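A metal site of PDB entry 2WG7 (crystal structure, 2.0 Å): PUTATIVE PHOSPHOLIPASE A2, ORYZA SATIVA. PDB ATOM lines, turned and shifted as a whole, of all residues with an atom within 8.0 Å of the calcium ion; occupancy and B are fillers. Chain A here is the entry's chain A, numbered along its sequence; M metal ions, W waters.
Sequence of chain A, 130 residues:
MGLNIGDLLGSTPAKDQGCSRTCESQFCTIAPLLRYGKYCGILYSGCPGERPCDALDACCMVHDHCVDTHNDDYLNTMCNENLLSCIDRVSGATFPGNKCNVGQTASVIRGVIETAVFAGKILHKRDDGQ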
ATOM      1  N   LEU A  34       2.125 -16.591 -28.692  1.00  0.00           N
ATOM      2  CA  LEU A  34       2.741 -17.067 -27.450  1.00  0.00           C
ATOM      3  C   LEU A  34       3.363 -18.450 -27.634  1.00  0.00           C
ATOM      4  O   LEU A  34       2.702 -19.360 -28.134  1.00  0.00           O
ATOM      5  CB  LEU A  34       1.659 -17.092 -26.366  1.00  0.00           C
ATOM      6  CG  LEU A  34       1.910 -17.430 -24.895  1.00  0.00           C
ATOM      7  CD1 LEU A  34       0.904 -16.679 -24.035  1.00  0.00           C
ATOM      8  CD2 LEU A  34       1.812 -18.920 -24.637  1.00  0.00           C
ATOM      9  N   TYR A  36       5.608 -20.855 -24.913  1.00  0.00           N
ATOM     10  CA  TYR A  36       6.127 -20.899 -23.546  1.00  0.00           C
ATOM     11  C   TYR A  36       6.368 -22.360 -23.168  1.00  0.00           C
ATOM     12  O   TYR A  36       5.485 -23.187 -23.311  1.00  0.00           O
ATOM     13  CB  TYR A  36       5.105 -20.250 -22.605  1.00  0.00           C
ATOM     14  CG  TYR A  36       5.414 -20.294 -21.116  1.00  0.00           C
ATOM     15  CD1 TYR A  36       5.797 -19.134 -20.433  1.00  0.00           C
ATOM     16  CD2 TYR A  36       5.294 -21.485 -20.390  1.00  0.00           C
ATOM     17  CE1 TYR A  36       6.066 -19.156 -19.082  1.00  0.00           C
ATOM     18  CE2 TYR A  36       5.574 -21.517 -19.018  1.00  0.00           C
ATOM     19  CZ  TYR A  36       5.954 -20.351 -18.371  1.00  0.00           C
ATOM     20  OH  TYR A  36       6.219 -20.357 -17.020  1.00  0.00           O
ATOM     21  N   LYS A  38       7.615 -26.093 -23.672  1.00  0.00           N
ATOM     22  CA  LYS A  38       7.576 -26.957 -24.851  1.00  0.00           C
ATOM     23  C   LYS A  38       6.142 -27.161 -25.370  1.00  0.00           C
ATOM     24  O   LYS A  38       5.953 -27.637 -26.488  1.00  0.00           O
ATOM     25  CB  LYS A  38       8.202 -28.324 -24.545  1.00  0.00           C
ATOM     26  CG  LYS A  38       9.664 -28.298 -24.112  1.00  0.00           C
ATOM     27  CD  LYS A  38      10.132 -29.720 -23.710  1.00  0.00           C
ATOM     28  CE  LYS A  38      11.517 -29.697 -23.091  1.00  0.00           C
ATOM     29  NZ  LYS A  38      11.869 -31.026 -22.478  1.00  0.00           N
ATOM     30  N   TYR A  39       5.154 -26.789 -24.550  1.00  0.00           N
ATOM     31  CA  TYR A  39       3.737 -27.113 -24.819  1.00  0.00           C
ATOM     32  C   TYR A  39       2.751 -25.934 -24.835  1.00  0.00           C
ATOM     33  O   TYR A  39       1.679 -26.044 -25.430  1.00  0.00           O
ATOM     34  CB  TYR A  39       3.224 -28.170 -23.818  1.00  0.00           C
ATOM     35  CG  TYR A  39       3.934 -29.516 -23.884  1.00  0.00           C
ATOM     36  CD1 TYR A  39       5.031 -29.783 -23.066  1.00  0.00           C
ATOM     37  CD2 TYR A  39       3.502 -30.512 -24.755  1.00  0.00           C
ATOM     38  CE1 TYR A  39       5.683 -31.026 -23.106  1.00  0.00           C
ATOM     39  CE2 TYR A  39       4.148 -31.769 -24.808  1.00  0.00           C
ATOM     40  CZ  TYR A  39       5.234 -32.009 -23.983  1.00  0.00           C
ATOM     41  OH  TYR A  39       5.874 -33.220 -24.036  1.00  0.00           O
ATOM     42  N   CYS A  40       3.061 -24.833 -24.151  1.00  0.00           N
ATOM     43  CA  CYS A  40       2.103 -23.732 -24.056  1.00  0.00           C
ATOM     44  C   CYS A  40       2.138 -22.858 -25.302  1.00  0.00           C
ATOM     45  O   CYS A  40       3.153 -22.229 -25.597  1.00  0.00           O
ATOM     46  CB  CYS A  40       2.326 -22.880 -22.797  1.00  0.00           C
ATOM     47  SG  CYS A  40       1.909 -23.665 -21.233  1.00  0.00           S
ATOM     48  N   GLY A  41       1.025 -22.827 -26.021  1.00  0.00           N
ATOM     49  CA  GLY A  41       0.896 -22.016 -27.220  1.00  0.00           C
ATOM     50  C   GLY A  41       0.030 -22.706 -28.256  1.00  0.00           C
ATOM     51  O   GLY A  41      -0.064 -23.936 -28.279  1.00  0.00           O
ATOM     52  N   ILE A  42      -0.619 -21.910 -29.107  1.00  0.00           N
ATOM     53  CA  ILE A  42      -1.487 -22.444 -30.151  1.00  0.00           C
ATOM     54  C   ILE A  42      -0.650 -23.085 -31.257  1.00  0.00           C
ATOM     55  O   ILE A  42       0.343 -22.508 -31.699  1.00  0.00           O
ATOM     56  CB  ILE A  42      -2.403 -21.323 -30.736  1.00  0.00           C
ATOM     57  CG1 ILE A  42      -3.332 -20.794 -29.640  1.00  0.00           C
ATOM     58  CG2 ILE A  42      -3.207 -21.834 -31.951  1.00  0.00           C
ATOM     59  CD1 ILE A  42      -3.739 -19.327 -29.801  1.00  0.00           C
ATOM     60  N   LEU A  43      -1.054 -24.292 -31.688  1.00  0.00           N
ATOM     61  CA  LEU A  43      -0.288 -25.053 -32.685  1.00  0.00           C
ATOM     62  C   LEU A  43       1.214 -25.061 -32.370  1.00  0.00           C
ATOM     63  O   LEU A  43       2.063 -24.755 -33.234  1.00  0.00           O
ATOM     64  CB  LEU A  43      -0.571 -24.539 -34.112  1.00  0.00           C
ATOM     65  CG  LEU A  43      -2.019 -24.572 -34.589  1.00  0.00           C
ATOM     66  CD1 LEU A  43      -2.190 -23.766 -35.869  1.00  0.00           C
ATOM     67  CD2 LEU A  43      -2.514 -25.998 -34.786  1.00  0.00           C
ATOM     68  N   TYR A  44       1.518 -25.397 -31.118  1.00  0.00           N
ATOM     69  CA  TYR A  44       2.874 -25.489 -30.609  1.00  0.00           C
ATOM     70  C   TYR A  44       2.844 -26.558 -29.510  1.00  0.00           C
ATOM     71  O   TYR A  44       2.150 -26.408 -28.506  1.00  0.00           O
ATOM     72  CB  TYR A  44       3.360 -24.138 -30.047  1.00  0.00           C
ATOM     73  CG  TYR A  44       4.694 -24.235 -29.328  1.00  0.00           C
ATOM     74  CD1 TYR A  44       5.881 -24.421 -30.051  1.00  0.00           C
ATOM     75  CD2 TYR A  44       4.770 -24.185 -27.936  1.00  0.00           C
ATOM     76  CE1 TYR A  44       7.111 -24.524 -29.400  1.00  0.00           C
ATOM     77  CE2 TYR A  44       5.994 -24.308 -27.277  1.00  0.00           C
ATOM     78  CZ  TYR A  44       7.153 -24.478 -28.018  1.00  0.00           C
ATOM     79  OH  TYR A  44       8.360 -24.611 -27.386  1.00  0.00           O
ATOM     80  N   SER A  45       3.571 -27.648 -29.723  1.00  0.00           N
ATOM     81  CA  SER A  45       3.572 -28.765 -28.784  1.00  0.00           C
ATOM     82  C   SER A  45       4.927 -29.475 -28.750  1.00  0.00           C
ATOM     83  O   SER A  45       5.717 -29.385 -29.697  1.00  0.00           O
ATOM     84  CB  SER A  45       2.446 -29.753 -29.118  1.00  0.00           C
ATOM     85  OG  SER A  45       1.900 -30.328 -27.935  1.00  0.00           O
ATOM     86  N   GLY A  46       5.184 -30.161 -27.644  1.00  0.00           N
ATOM     87  CA  GLY A  46       6.447 -30.855 -27.437  1.00  0.00           C
ATOM     88  C   GLY A  46       6.469 -32.248 -28.061  1.00  0.00           C
ATOM     89  O   GLY A  46       5.424 -32.883 -28.238  1.00  0.00           O
ATOM     90  N   ASP A  57       3.721 -25.276 -17.978  1.00  0.00           N
ATOM     91  CA  ASP A  57       3.979 -26.068 -19.183  1.00  0.00           C
ATOM     92  C   ASP A  57       3.338 -27.454 -19.074  1.00  0.00           C
ATOM     93  O   ASP A  57       2.822 -28.003 -20.050  1.00  0.00           O
ATOM     94  CB  ASP A  57       5.490 -26.201 -19.402  1.00  0.00           C
ATOM     95  CG  ASP A  57       5.852 -26.546 -20.837  1.00  0.00           C
ATOM     96  OD1 ASP A  57       5.054 -26.234 -21.772  1.00  0.00           O
ATOM     97  OD2 ASP A  57       6.955 -27.118 -21.027  1.00  0.00           O
ATOM     98  N   CYS A  60      -0.335 -27.246 -19.933  1.00  0.00           N
ATOM     99  CA  CYS A  60      -0.481 -27.202 -21.390  1.00  0.00           C
ATOM    100  C   CYS A  60      -0.228 -28.555 -22.068  1.00  0.00           C
ATOM    101  O   CYS A  60      -0.900 -28.904 -23.043  1.00  0.00           O
ATOM    102  CB  CYS A  60       0.423 -26.143 -22.000  1.00  0.00           C
ATOM    103  SG  CYS A  60       0.053 -24.454 -21.478  1.00  0.00           S
ATOM    104  N   MET A  61       0.741 -29.308 -21.536  1.00  0.00           N
ATOM    105  CA  MET A  61       1.044 -30.661 -22.041  1.00  0.00           C
ATOM    106  C   MET A  61      -0.193 -31.570 -21.960  1.00  0.00           C
ATOM    107  O   MET A  61      -0.529 -32.245 -22.931  1.00  0.00           O
ATOM    108  CB  MET A  61       2.234 -31.267 -21.279  1.00  0.00           C
ATOM    109  CG  MET A  61       2.537 -32.738 -21.605  1.00  0.00           C
ATOM    110  SD  MET A  61       3.763 -33.412 -20.477  1.00  0.00           S
ATOM    111  CE  MET A  61       2.859 -33.422 -18.949  1.00  0.00           C
ATOM    112  N   HIS A  63      -3.391 -30.636 -21.691  1.00  0.00           N
ATOM    113  CA  HIS A  63      -4.387 -30.064 -22.609  1.00  0.00           C
ATOM    114  C   HIS A  63      -4.134 -30.442 -24.068  1.00  0.00           C
ATOM    115  O   HIS A  63      -5.076 -30.830 -24.765  1.00  0.00           O
ATOM    116  CB  HIS A  63      -4.425 -28.539 -22.454  1.00  0.00           C
ATOM    117  CG  HIS A  63      -5.407 -27.867 -23.360  1.00  0.00           C
ATOM    118  ND1 HIS A  63      -5.050 -27.366 -24.594  1.00  0.00           N
ATOM    119  CD2 HIS A  63      -6.722 -27.600 -23.215  1.00  0.00           C
ATOM    120  CE1 HIS A  63      -6.108 -26.832 -25.177  1.00  0.00           C
ATOM    121  NE2 HIS A  63      -7.131 -26.948 -24.353  1.00  0.00           N
ATOM    122  N   ASP A  64      -2.894 -30.297 -24.523  1.00  0.00           N
ATOM    123  CA  ASP A  64      -2.512 -30.631 -25.904  1.00  0.00           C
ATOM    124  C   ASP A  64      -2.839 -32.082 -26.241  1.00  0.00           C
ATOM    125  O   ASP A  64      -3.434 -32.370 -27.282  1.00  0.00           O
ATOM    126  CB  ASP A  64      -1.028 -30.391 -26.146  1.00  0.00           C
ATOM    127  CG  ASP A  64      -0.689 -28.915 -26.288  1.00  0.00           C
ATOM    128  OD1 ASP A  64      -1.592 -28.070 -26.166  1.00  0.00           O
ATOM    129  OD2 ASP A  64       0.497 -28.592 -26.512  1.00  0.00           O
ATOM    130  N   HIS A  65      -2.454 -32.984 -25.346  1.00  0.00           N
ATOM    131  CA  HIS A  65      -2.802 -34.397 -25.502  1.00  0.00           C
ATOM    132  C   HIS A  65      -4.311 -34.629 -25.422  1.00  0.00           C
ATOM    133  O   HIS A  65      -4.845 -35.416 -26.207  1.00  0.00           O
ATOM    134  CB  HIS A  65      -2.044 -35.266 -24.491  1.00  0.00           C
ATOM    135  CG  HIS A  65      -0.583 -35.395 -24.796  1.00  0.00           C
ATOM    136  ND1 HIS A  65      -0.100 -36.298 -25.718  1.00  0.00           N
ATOM    137  CD2 HIS A  65       0.483 -34.723 -24.323  1.00  0.00           C
ATOM    138  CE1 HIS A  65       1.214 -36.174 -25.798  1.00  0.00           C
ATOM    139  NE2 HIS A  65       1.594 -35.230 -24.955  1.00  0.00           N
HETATM  140 CA    CA M   1       0.247 -26.209 -27.272  1.00  0.00          CA
HETATM  141  O   HOH W   1      -0.784 -26.844 -29.364  1.00  0.00           O
HETATM  142  O   HOH W   2      -1.292 -24.884 -25.431  1.00  0.00           O
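SG of Cys 40 forms a disulfide with SG of Cys 60 (2.0 Å). The backbone NH of Tyr 39 sits at hydrogen-bond distance from the side-chain carboxylate of Asp 57, at 2.8 Å. The side-chain carboxylate (OD2) of Asp 64 lies close to the side-chain hydroxyl (OG) of Ser 45 (2.6 Å).
Of the 17 residues printed, 4 come within 4 Å of the calcium ion.
The calcium ion is bound by the backbone carbonyl oxygen (O) of Tyr 44 (2.3 Å). O of Tyr 39 is bound to the calcium ion (2.3 Å). Water W1 binds the calcium ion (2.4 Å). The calcium ion is bound by O of Gly 41 (2.5 Å). OD2 of Asp 64 is bound to the calcium ion. Water W2 binds the calcium ion (2.7 Å). OD1 of Asp 64 is bound to the calcium ion, at 2.8 Å.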
